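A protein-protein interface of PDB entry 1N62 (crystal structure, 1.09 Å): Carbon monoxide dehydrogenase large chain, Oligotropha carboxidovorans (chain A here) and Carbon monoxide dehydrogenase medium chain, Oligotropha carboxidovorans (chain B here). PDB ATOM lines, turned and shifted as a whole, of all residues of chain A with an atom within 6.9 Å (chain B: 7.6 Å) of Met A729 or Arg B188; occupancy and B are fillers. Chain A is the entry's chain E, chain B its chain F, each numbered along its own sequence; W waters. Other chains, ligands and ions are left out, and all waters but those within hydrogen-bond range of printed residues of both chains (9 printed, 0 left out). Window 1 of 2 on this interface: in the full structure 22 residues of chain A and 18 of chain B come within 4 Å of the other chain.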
ATOM      1  N   MET A 302     -13.576  16.998 -15.415  1.00  0.00           N
ATOM      2  CA  MET A 302     -12.796  16.410 -14.359  1.00  0.00           C
ATOM      3  C   MET A 302     -11.584  15.695 -14.922  1.00  0.00           C
ATOM      4  O   MET A 302     -10.530  15.744 -14.351  1.00  0.00           O
ATOM      5  CB  MET A 302     -13.643  15.481 -13.542  1.00  0.00           C
ATOM      6  CG  MET A 302     -14.648  16.222 -12.686  1.00  0.00           C
ATOM      7  SD  MET A 302     -15.618  15.047 -11.811  1.00  0.00           S
ATOM      8  CE  MET A 302     -17.041  15.995 -11.501  1.00  0.00           C
ATOM      9  N   GLY A 712      -6.268  31.462  -5.698  1.00  0.00           N
ATOM     10  CA  GLY A 712      -7.143  30.348  -5.401  1.00  0.00           C
ATOM     11  C   GLY A 712      -6.857  29.052  -6.097  1.00  0.00           C
ATOM     12  O   GLY A 712      -7.225  28.029  -5.563  1.00  0.00           O
ATOM     13  N   GLU A 714      -5.724  25.632  -7.734  1.00  0.00           N
ATOM     14  CA  GLU A 714      -4.784  24.590  -7.400  1.00  0.00           C
ATOM     15  C   GLU A 714      -5.301  23.279  -7.904  1.00  0.00           C
ATOM     16  O   GLU A 714      -6.493  23.068  -7.932  1.00  0.00           O
ATOM     17  CB  GLU A 714      -4.577  24.487  -5.883  1.00  0.00           C
ATOM     18  CG  GLU A 714      -5.860  24.285  -5.140  1.00  0.00           C
ATOM     19  CD  GLU A 714      -5.683  24.382  -3.638  1.00  0.00           C
ATOM     20  OE1 GLU A 714      -4.528  24.438  -3.145  1.00  0.00           O
ATOM     21  OE2 GLU A 714      -6.706  24.256  -2.938  1.00  0.00           O
ATOM     22  N   ARG A 716      -4.307  19.485  -6.385  1.00  0.00           N
ATOM     23  CA  ARG A 716      -3.488  18.863  -5.375  1.00  0.00           C
ATOM     24  C   ARG A 716      -3.614  17.394  -5.418  1.00  0.00           C
ATOM     25  O   ARG A 716      -4.521  16.870  -6.021  1.00  0.00           O
ATOM     26  CB  ARG A 716      -3.908  19.346  -3.988  1.00  0.00           C
ATOM     27  CG  ARG A 716      -3.778  20.850  -3.774  1.00  0.00           C
ATOM     28  CD  ARG A 716      -4.771  21.419  -2.780  1.00  0.00           C
ATOM     29  NE  ARG A 716      -6.094  20.823  -2.933  1.00  0.00           N
ATOM     30  CZ  ARG A 716      -7.005  20.772  -1.972  1.00  0.00           C
ATOM     31  NH1 ARG A 716      -7.338  21.882  -1.331  1.00  0.00           N
ATOM     32  NH2 ARG A 716      -7.346  19.601  -1.453  1.00  0.00           N
ATOM     33  N   GLY A 725      -9.497  18.562  -5.879  1.00  0.00           N
ATOM     34  CA  GLY A 725      -9.900  19.842  -6.367  1.00  0.00           C
ATOM     35  C   GLY A 725      -9.979  19.966  -7.874  1.00  0.00           C
ATOM     36  O   GLY A 725     -10.150  21.065  -8.363  1.00  0.00           O
ATOM     37  N   ALA A 726      -9.982  18.846  -8.579  1.00  0.00           N
ATOM     38  CA  ALA A 726      -9.922  18.850 -10.037  1.00  0.00           C
ATOM     39  C   ALA A 726     -11.312  18.811 -10.641  1.00  0.00           C
ATOM     40  O   ALA A 726     -11.670  17.910 -11.399  1.00  0.00           O
ATOM     41  CB  ALA A 726      -9.081  17.713 -10.545  1.00  0.00           C
ATOM     42  N   SER A 727     -12.124  19.776 -10.242  1.00  0.00           N
ATOM     43  CA  SER A 727     -13.381  20.075 -10.862  1.00  0.00           C
ATOM     44  C   SER A 727     -13.730  21.509 -10.516  1.00  0.00           C
ATOM     45  O   SER A 727     -13.153  22.093  -9.627  1.00  0.00           O
ATOM     46  CB  SER A 727     -14.454  19.158 -10.299  1.00  0.00           C
ATOM     47  OG  SER A 727     -14.995  19.667  -9.087  1.00  0.00           O
ATOM     48  N   PHE A 728     -14.729  22.040 -11.180  1.00  0.00           N
ATOM     49  CA  PHE A 728     -15.097  23.388 -10.912  1.00  0.00           C
ATOM     50  C   PHE A 728     -15.844  23.547  -9.604  1.00  0.00           C
ATOM     51  O   PHE A 728     -16.152  24.650  -9.219  1.00  0.00           O
ATOM     52  CB  PHE A 728     -15.907  23.973 -12.062  1.00  0.00           C
ATOM     53  CG  PHE A 728     -15.117  24.224 -13.330  1.00  0.00           C
ATOM     54  CD1 PHE A 728     -13.761  24.166 -13.365  1.00  0.00           C
ATOM     55  CD2 PHE A 728     -15.769  24.513 -14.515  1.00  0.00           C
ATOM     56  CE1 PHE A 728     -13.065  24.388 -14.522  1.00  0.00           C
ATOM     57  CE2 PHE A 728     -15.072  24.809 -15.658  1.00  0.00           C
ATOM     58  CZ  PHE A 728     -13.752  24.698 -15.684  1.00  0.00           C
ATOM     59  N   MET A 729     -16.076  22.453  -8.891  1.00  0.00           N
ATOM     60  CA  MET A 729     -16.502  22.597  -7.500  1.00  0.00           C
ATOM     61  C   MET A 729     -15.481  23.326  -6.679  1.00  0.00           C
ATOM     62  O   MET A 729     -15.828  23.963  -5.696  1.00  0.00           O
ATOM     63  CB  MET A 729     -16.761  21.233  -6.858  1.00  0.00           C
ATOM     64  CG  MET A 729     -17.870  20.411  -7.495  1.00  0.00           C
ATOM     65  SD  MET A 729     -19.526  20.984  -7.095  1.00  0.00           S
ATOM     66  CE  MET A 729     -19.231  21.889  -5.593  1.00  0.00           C
ATOM     67  N   ASP A 730     -14.219  23.110  -6.986  1.00  0.00           N
ATOM     68  CA  ASP A 730     -13.147  23.605  -6.166  1.00  0.00           C
ATOM     69  C   ASP A 730     -12.158  24.444  -6.939  1.00  0.00           C
ATOM     70  O   ASP A 730     -11.536  25.280  -6.342  1.00  0.00           O
ATOM     71  CB  ASP A 730     -12.413  22.468  -5.532  1.00  0.00           C
ATOM     72  CG  ASP A 730     -13.258  21.742  -4.583  1.00  0.00           C
ATOM     73  OD1 ASP A 730     -13.556  22.311  -3.498  1.00  0.00           O
ATOM     74  OD2 ASP A 730     -13.734  20.644  -4.885  1.00  0.00           O
ATOM     75  N   PHE A 731     -11.940  24.133  -8.205  1.00  0.00           N
ATOM     76  CA  PHE A 731     -10.909  24.800  -8.971  1.00  0.00           C
ATOM     77  C   PHE A 731     -11.327  26.228  -9.219  1.00  0.00           C
ATOM     78  O   PHE A 731     -12.326  26.474  -9.865  1.00  0.00           O
ATOM     79  CB  PHE A 731     -10.730  24.051 -10.272  1.00  0.00           C
ATOM     80  CG  PHE A 731      -9.602  24.534 -11.077  1.00  0.00           C
ATOM     81  CD1 PHE A 731      -8.321  24.118 -10.783  1.00  0.00           C
ATOM     82  CD2 PHE A 731      -9.820  25.296 -12.213  1.00  0.00           C
ATOM     83  CE1 PHE A 731      -7.273  24.626 -11.496  1.00  0.00           C
ATOM     84  CE2 PHE A 731      -8.772  25.733 -12.980  1.00  0.00           C
ATOM     85  CZ  PHE A 731      -7.514  25.374 -12.643  1.00  0.00           C
ATOM     86  N   PHE A 732     -10.586  27.177  -8.703  1.00  0.00           N
ATOM     87  CA  PHE A 732     -11.023  28.542  -8.677  1.00  0.00           C
ATOM     88  C   PHE A 732     -10.905  29.161 -10.057  1.00  0.00           C
ATOM     89  O   PHE A 732      -9.866  29.548 -10.499  1.00  0.00           O
ATOM     90  CB  PHE A 732     -10.157  29.323  -7.685  1.00  0.00           C
ATOM     91  CG  PHE A 732     -10.522  30.736  -7.564  1.00  0.00           C
ATOM     92  CD1 PHE A 732     -11.713  31.116  -7.012  1.00  0.00           C
ATOM     93  CD2 PHE A 732      -9.646  31.706  -7.924  1.00  0.00           C
ATOM     94  CE1 PHE A 732     -12.028  32.453  -6.831  1.00  0.00           C
ATOM     95  CE2 PHE A 732      -9.960  33.033  -7.744  1.00  0.00           C
ATOM     96  CZ  PHE A 732     -11.190  33.399  -7.243  1.00  0.00           C
ATOM     97  N   GLU A 738     -15.865  38.084  -8.953  1.00  0.00           N
ATOM     98  CA  GLU A 738     -14.574  38.066  -8.292  1.00  0.00           C
ATOM     99  C   GLU A 738     -13.523  38.801  -9.112  1.00  0.00           C
ATOM    100  O   GLU A 738     -12.512  39.164  -8.568  1.00  0.00           O
ATOM    101  CB  GLU A 738     -14.073  36.648  -8.044  1.00  0.00           C
ATOM    102  CG  GLU A 738     -14.895  35.876  -7.057  1.00  0.00           C
ATOM    103  CD  GLU A 738     -16.176  35.368  -7.668  1.00  0.00           C
ATOM    104  OE1 GLU A 738     -16.159  35.005  -8.860  1.00  0.00           O
ATOM    105  OE2 GLU A 738     -17.156  35.220  -6.922  1.00  0.00           O
ATOM    106  N   ASP A 794      -5.688  32.086  -0.927  1.00  0.00           N
ATOM    107  CA  ASP A 794      -7.089  32.033  -0.652  1.00  0.00           C
ATOM    108  C   ASP A 794      -7.336  32.266   0.814  1.00  0.00           C
ATOM    109  O   ASP A 794      -6.433  32.455   1.606  1.00  0.00           O
ATOM    110  CB  ASP A 794      -7.717  30.780  -1.183  1.00  0.00           C
ATOM    111  CG  ASP A 794      -7.218  29.549  -0.542  1.00  0.00           C
ATOM    112  OD1 ASP A 794      -6.313  29.606   0.324  1.00  0.00           O
ATOM    113  OD2 ASP A 794      -7.663  28.441  -0.948  1.00  0.00           O
ATOM    114  N   ALA A 795      -8.594  32.320   1.172  1.00  0.00           N
ATOM    115  CA  ALA A 795      -8.920  32.885   2.471  1.00  0.00           C
ATOM    116  C   ALA A 795      -8.462  31.996   3.595  1.00  0.00           C
ATOM    117  O   ALA A 795      -7.925  32.496   4.576  1.00  0.00           O
ATOM    118  CB  ALA A 795     -10.380  33.166   2.564  1.00  0.00           C
ATOM    119  N   TRP A 796      -8.575  30.678   3.468  1.00  0.00           N
ATOM    120  CA  TRP A 796      -8.166  29.851   4.580  1.00  0.00           C
ATOM    121  C   TRP A 796      -6.680  29.963   4.782  1.00  0.00           C
ATOM    122  O   TRP A 796      -6.208  29.930   5.907  1.00  0.00           O
ATOM    123  CB  TRP A 796      -8.617  28.394   4.474  1.00  0.00           C
ATOM    124  CG  TRP A 796      -7.900  27.501   3.539  1.00  0.00           C
ATOM    125  CD1 TRP A 796      -8.294  27.188   2.290  1.00  0.00           C
ATOM    126  CD2 TRP A 796      -6.718  26.747   3.782  1.00  0.00           C
ATOM    127  NE1 TRP A 796      -7.470  26.239   1.749  1.00  0.00           N
ATOM    128  CE2 TRP A 796      -6.480  25.962   2.641  1.00  0.00           C
ATOM    129  CE3 TRP A 796      -5.868  26.597   4.878  1.00  0.00           C
ATOM    130  CZ2 TRP A 796      -5.439  25.054   2.560  1.00  0.00           C
ATOM    131  CZ3 TRP A 796      -4.821  25.731   4.785  1.00  0.00           C
ATOM    132  CH2 TRP A 796      -4.612  24.959   3.635  1.00  0.00           C
ATOM    133  N   PRO B  39     -26.770  16.940 -10.819  1.00  0.00           N
ATOM    134  CA  PRO B  39     -25.326  16.883 -10.722  1.00  0.00           C
ATOM    135  C   PRO B  39     -24.826  15.587 -10.115  1.00  0.00           C
ATOM    136  O   PRO B  39     -23.827  15.063 -10.618  1.00  0.00           O
ATOM    137  CB  PRO B  39     -24.998  18.091  -9.877  1.00  0.00           C
ATOM    138  CG  PRO B  39     -26.025  19.094 -10.298  1.00  0.00           C
ATOM    139  CD  PRO B  39     -27.300  18.268 -10.460  1.00  0.00           C
ATOM    140  N   LYS B 185     -22.491  34.992   4.588  1.00  0.00           N
ATOM    141  CA  LYS B 185     -21.910  33.809   4.021  1.00  0.00           C
ATOM    142  C   LYS B 185     -20.507  34.102   3.575  1.00  0.00           C
ATOM    143  O   LYS B 185     -20.240  35.099   2.915  1.00  0.00           O
ATOM    144  CB  LYS B 185     -22.716  33.377   2.826  1.00  0.00           C
ATOM    145  CG  LYS B 185     -22.226  32.131   2.118  1.00  0.00           C
ATOM    146  CD  LYS B 185     -23.228  31.662   1.099  1.00  0.00           C
ATOM    147  CE  LYS B 185     -22.751  30.472   0.292  1.00  0.00           C
ATOM    148  NZ  LYS B 185     -23.784  30.003  -0.607  1.00  0.00           N
ATOM    149  N   LEU B 186     -19.620  33.187   3.879  1.00  0.00           N
ATOM    150  CA  LEU B 186     -18.254  33.217   3.420  1.00  0.00           C
ATOM    151  C   LEU B 186     -18.099  32.096   2.436  1.00  0.00           C
ATOM    152  O   LEU B 186     -18.462  30.979   2.739  1.00  0.00           O
ATOM    153  CB  LEU B 186     -17.335  33.008   4.606  1.00  0.00           C
ATOM    154  CG  LEU B 186     -15.871  32.975   4.265  1.00  0.00           C
ATOM    155  CD1 LEU B 186     -15.400  34.296   3.709  1.00  0.00           C
ATOM    156  CD2 LEU B 186     -15.064  32.596   5.464  1.00  0.00           C
ATOM    157  N   LYS B 187     -17.613  32.423   1.249  1.00  0.00           N
ATOM    158  CA  LYS B 187     -17.494  31.419   0.220  1.00  0.00           C
ATOM    159  C   LYS B 187     -16.311  31.738  -0.654  1.00  0.00           C
ATOM    160  O   LYS B 187     -15.834  32.851  -0.658  1.00  0.00           O
ATOM    161  CB  LYS B 187     -18.749  31.342  -0.626  1.00  0.00           C
ATOM    162  CG  LYS B 187     -19.091  32.645  -1.325  1.00  0.00           C
ATOM    163  CD  LYS B 187     -20.501  32.658  -1.846  1.00  0.00           C
ATOM    164  CE  LYS B 187     -20.725  33.784  -2.823  1.00  0.00           C
ATOM    165  NZ  LYS B 187     -20.537  35.110  -2.198  1.00  0.00           N
ATOM    166  N   ARG B 188     -15.878  30.776  -1.448  1.00  0.00           N
ATOM    167  CA  ARG B 188     -14.712  30.995  -2.285  1.00  0.00           C
ATOM    168  C   ARG B 188     -15.025  31.840  -3.501  1.00  0.00           C
ATOM    169  O   ARG B 188     -14.144  32.481  -4.035  1.00  0.00           O
ATOM    170  CB  ARG B 188     -14.113  29.671  -2.709  1.00  0.00           C
ATOM    171  CG  ARG B 188     -13.431  28.943  -1.575  1.00  0.00           C
ATOM    172  CD  ARG B 188     -12.965  27.559  -1.901  1.00  0.00           C
ATOM    173  NE  ARG B 188     -14.107  26.729  -2.229  1.00  0.00           N
ATOM    174  CZ  ARG B 188     -14.014  25.469  -2.558  1.00  0.00           C
ATOM    175  NH1 ARG B 188     -12.846  24.872  -2.691  1.00  0.00           N
ATOM    176  NH2 ARG B 188     -15.107  24.809  -2.794  1.00  0.00           N
ATOM    177  N   LYS B 189     -16.246  31.760  -4.000  1.00  0.00           N
ATOM    178  CA  LYS B 189     -16.654  32.469  -5.182  1.00  0.00           C
ATOM    179  C   LYS B 189     -18.134  32.291  -5.290  1.00  0.00           C
ATOM    180  O   LYS B 189     -18.721  31.458  -4.604  1.00  0.00           O
ATOM    181  CB  LYS B 189     -15.975  31.944  -6.454  1.00  0.00           C
ATOM    182  CG  LYS B 189     -15.976  30.443  -6.592  1.00  0.00           C
ATOM    183  CD  LYS B 189     -15.482  29.942  -7.910  1.00  0.00           C
ATOM    184  CE  LYS B 189     -16.559  29.921  -8.921  1.00  0.00           C
ATOM    185  NZ  LYS B 189     -16.067  29.345 -10.209  1.00  0.00           N
ATOM    186  N   ILE B 190     -18.734  33.070  -6.160  1.00  0.00           N
ATOM    187  CA  ILE B 190     -20.095  32.840  -6.592  1.00  0.00           C
ATOM    188  C   ILE B 190     -20.301  31.377  -6.825  1.00  0.00           C
ATOM    189  O   ILE B 190     -19.575  30.719  -7.550  1.00  0.00           O
ATOM    190  CB  ILE B 190     -20.418  33.637  -7.909  1.00  0.00           C
ATOM    191  CG1 ILE B 190     -20.404  35.120  -7.608  1.00  0.00           C
ATOM    192  CG2 ILE B 190     -21.753  33.215  -8.482  1.00  0.00           C
ATOM    193  CD1 ILE B 190     -21.449  35.581  -6.631  1.00  0.00           C
ATOM    194  N   GLY B 191     -21.402  30.919  -6.276  1.00  0.00           N
ATOM    195  CA  GLY B 191     -21.866  29.591  -6.511  1.00  0.00           C
ATOM    196  C   GLY B 191     -21.351  28.622  -5.490  1.00  0.00           C
ATOM    197  O   GLY B 191     -21.799  27.520  -5.458  1.00  0.00           O
ATOM    198  N   ASP B 192     -20.314  28.954  -4.762  1.00  0.00           N
ATOM    199  CA  ASP B 192     -19.713  27.988  -3.856  1.00  0.00           C
ATOM    200  C   ASP B 192     -20.570  27.858  -2.611  1.00  0.00           C
ATOM    201  O   ASP B 192     -21.124  28.809  -2.075  1.00  0.00           O
ATOM    202  CB  ASP B 192     -18.332  28.472  -3.483  1.00  0.00           C
ATOM    203  CG  ASP B 192     -17.489  27.511  -2.691  1.00  0.00           C
ATOM    204  OD1 ASP B 192     -17.647  26.275  -2.828  1.00  0.00           O
ATOM    205  OD2 ASP B 192     -16.608  27.972  -1.907  1.00  0.00           O
ATOM    206  N   TYR B 193     -20.652  26.643  -2.122  1.00  0.00           N
ATOM    207  CA  TYR B 193     -21.235  26.389  -0.818  1.00  0.00           C
ATOM    208  C   TYR B 193     -20.337  27.019   0.237  1.00  0.00           C
ATOM    209  O   TYR B 193     -19.119  27.157   0.044  1.00  0.00           O
ATOM    210  CB  TYR B 193     -21.293  24.906  -0.580  1.00  0.00           C
ATOM    211  CG  TYR B 193     -22.110  24.194  -1.584  1.00  0.00           C
ATOM    212  CD1 TYR B 193     -23.492  24.258  -1.546  1.00  0.00           C
ATOM    213  CD2 TYR B 193     -21.506  23.544  -2.648  1.00  0.00           C
ATOM    214  CE1 TYR B 193     -24.218  23.640  -2.471  1.00  0.00           C
ATOM    215  CE2 TYR B 193     -22.248  23.038  -3.652  1.00  0.00           C
ATOM    216  CZ  TYR B 193     -23.593  23.022  -3.526  1.00  0.00           C
ATOM    217  OH  TYR B 193     -24.346  22.411  -4.477  1.00  0.00           O
ATOM    218  N   ALA B 194     -20.957  27.405   1.338  1.00  0.00           N
ATOM    219  CA  ALA B 194     -20.288  28.235   2.315  1.00  0.00           C
ATOM    220  C   ALA B 194     -19.105  27.515   2.884  1.00  0.00           C
ATOM    221  O   ALA B 194     -19.192  26.393   3.372  1.00  0.00           O
ATOM    222  CB  ALA B 194     -21.209  28.603   3.410  1.00  0.00           C
ATOM    223  N   THR B 195     -18.037  28.267   3.040  1.00  0.00           N
ATOM    224  CA  THR B 195     -17.038  27.933   4.020  1.00  0.00           C
ATOM    225  C   THR B 195     -17.653  27.919   5.409  1.00  0.00           C
ATOM    226  O   THR B 195     -17.420  27.010   6.200  1.00  0.00           O
ATOM    227  CB  THR B 195     -15.971  28.990   3.919  1.00  0.00           C
ATOM    228  OG1 THR B 195     -15.413  28.925   2.578  1.00  0.00           O
ATOM    229  CG2 THR B 195     -14.870  28.731   4.912  1.00  0.00           C
ATOM    230  N   ASP B 259     -11.922  20.605   3.828  1.00  0.00           N
ATOM    231  CA  ASP B 259     -11.943  20.385   2.406  1.00  0.00           C
ATOM    232  C   ASP B 259     -11.313  21.573   1.710  1.00  0.00           C
ATOM    233  O   ASP B 259     -10.475  22.250   2.296  1.00  0.00           O
ATOM    234  CB  ASP B 259     -13.370  20.033   1.934  1.00  0.00           C
ATOM    235  CG  ASP B 259     -14.378  21.134   2.121  1.00  0.00           C
ATOM    236  OD1 ASP B 259     -14.047  22.333   2.090  1.00  0.00           O
ATOM    237  OD2 ASP B 259     -15.568  20.871   2.333  1.00  0.00           O
ATOM    238  N   GLY B 260     -11.633  21.781   0.455  1.00  0.00           N
ATOM    239  CA  GLY B 260     -11.043  22.871  -0.290  1.00  0.00           C
ATOM    240  C   GLY B 260     -11.338  24.240   0.276  1.00  0.00           C
ATOM    241  O   GLY B 260     -10.632  25.179  -0.039  1.00  0.00           O
ATOM    242  N   ARG B 261     -12.361  24.347   1.106  1.00  0.00           N
ATOM    243  CA  ARG B 261     -12.689  25.587   1.739  1.00  0.00           C
ATOM    244  C   ARG B 261     -11.838  25.848   2.946  1.00  0.00           C
ATOM    245  O   ARG B 261     -11.877  26.935   3.528  1.00  0.00           O
ATOM    246  CB  ARG B 261     -14.148  25.600   2.121  1.00  0.00           C
ATOM    247  CG  ARG B 261     -15.052  25.503   0.940  1.00  0.00           C
ATOM    248  CD  ARG B 261     -16.475  25.234   1.335  1.00  0.00           C
ATOM    249  NE  ARG B 261     -17.276  24.930   0.175  1.00  0.00           N
ATOM    250  CZ  ARG B 261     -17.234  23.787  -0.477  1.00  0.00           C
ATOM    251  NH1 ARG B 261     -16.527  22.768  -0.028  1.00  0.00           N
ATOM    252  NH2 ARG B 261     -17.882  23.670  -1.603  1.00  0.00           N
ATOM    253  N   GLY B 262     -11.040  24.860   3.308  1.00  0.00           N
ATOM    254  CA  GLY B 262     -10.150  25.011   4.430  1.00  0.00           C
ATOM    255  C   GLY B 262     -10.444  23.990   5.487  1.00  0.00           C
ATOM    256  O   GLY B 262     -11.345  23.183   5.375  1.00  0.00           O
HETATM  257  O   HOH W   1     -22.663  22.603  -6.837  1.00  0.00           O
HETATM  258  O   HOH W   2      -7.651  22.578   1.368  1.00  0.00           O
HETATM  259  O   HOH W   3     -10.290  27.917  -0.345  1.00  0.00           O
HETATM  260  O   HOH W   4     -10.296  25.689  -3.275  1.00  0.00           O
HETATM  261  O   HOH W   5     -15.351  27.093  -5.435  1.00  0.00           O
HETATM  262  O   HOH W   6     -13.335  20.659  -1.425  1.00  0.00           O
HETATM  263  O   HOH W   7      -8.027  24.555  -0.583  1.00  0.00           O
HETATM  264  O   HOH W   8     -18.382  24.405  -4.732  1.00  0.00           O
HETATM  265  O   HOH W   9     -14.870  26.867 -10.272  1.00  0.00           O
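Arg A716 touches Gly B260 (NH1 to CA, 3.97 Å). Met A729 touches Tyr B193 (CE to CE2, 3.8 Å). Phe A732 touches Arg B188. Lys B189 touches Phe A732 (CB to CE1, 3.998 Å). Glu A738 touches Lys B189 (OE2 to CA, 3.3 Å). NE1 of Trp A796 touches O of Gly B260, 3.8 Å away. Trp A796 touches Arg B261 (CB to O, 3.7 Å). Gly B262 touches Trp A796 (CA to CG, 3.5 Å).
The backbone carbonyl oxygen of Met A729 is in hydrogen-bond range of the guanidinium group of Arg B188 (3.1 Å). The guanidinium group (NH1) of Arg B188 is in salt-bridge range of the side-chain carboxylate (OD1) of Asp A730 (2.8 Å). The side-chain carboxylate (OE2) of Glu A738 sits at hydrogen-bond distance from the backbone NH (N) of Ile B190.
Water W9 lies within hydrogen-bond range of the backbone carbonyl oxygen of Phe A731 (2.6 Å), the side-chain amino group of Lys B189 (2.8 Å) and the backbone carbonyl oxygen of Phe A728 (2.8 Å). Water W6 bridges OD1 of Asp A730 and N of Gly B260. Water W4 lies within hydrogen-bond range of NH1 of Arg B188 (2.7 Å), O of Gly B260 (3.3 Å) and O of Asp A730 (3.3 Å). Water W8 lies within hydrogen-bond range of the backbone carbonyl oxygen (O) of Met A729 (2.8 Å), the side-chain carboxylate (OD1) of Asp B192 (2.8 Å) and the guanidinium group (NH2) of Arg B261 (3.3 Å). Water W2 bridges the guanidinium group (NH1) of Arg A716 (2.8 Å) and the backbone carbonyl oxygen (O) of Asp B259 (3.0 Å). Water W5 lies within hydrogen-bond range of O of Met A729 and NE of Arg B188.
NH1 of Arg A716 is in salt-bridge range of OE2 of Glu A714, 2.9 Å away. N of Met A729 is in hydrogen-bond range of OG of Ser A727 (3.0 Å). The side-chain carboxylate of Asp A794 lies within hydrogen-bond range of the indole nitrogen of Trp A796 (3.5 Å). The backbone carbonyl oxygen of Gly B260 lies close to the guanidinium group of Arg B188 (3.5 Å). The guanidinium group of Arg B261 is in hydrogen-bond range of the backbone carbonyl oxygen of Tyr B193 (2.9 Å). OD2 of Asp B259 is in salt-bridge range of NH1 of Arg B261 (3.2 Å).
Printed residues of chain B within 4 Å of Met A729: Arg B188 (3.1 Å) and Tyr B193 (3.8 Å). Printed residues of chain A within 4 Å of Arg B188: Met A729, Asp A730 and Phe A732. Of the printed residues of chain B, Arg A716 touches Gly B260 (3.97 Å). Printed residues of chain A within 4 Å of Arg B261: Trp A796. Phe A731 touches none of the printed residues of chain B. The nearest printed residue of chain B that does not touch Met A729 is Asp B192 (4.1 Å).
Of the 16 printed residues of chain B, 7 touch a printed residue of chain A. Hydrophobic or aromatic side chains of chain B within 4 Å of the printed part of chain A: Ile B190 and Tyr B193. Of the 16 printed residues of chain A, 6 touch a printed residue of chain B. Printed residues of chain A that touch a printed residue of chain B: Arg A716, Met A729, Asp A730, Phe A732, Glu A738 and Trp A796. Hydrophobic or aromatic side chains of chain A that line the printed part of chain B: Met A729, Phe A732 and Trp A796. Along chain A the printed residues that touch a printed residue of chain B span positions 716 to 796. Among the printed residues, 11 pairs touch across the chains. Among the printed residues, Asp or Glu carboxylates within 4 Å of a Lys or Arg side-chain nitrogen of the other chain: Asp A730 with Arg B188 (2.8 Å).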
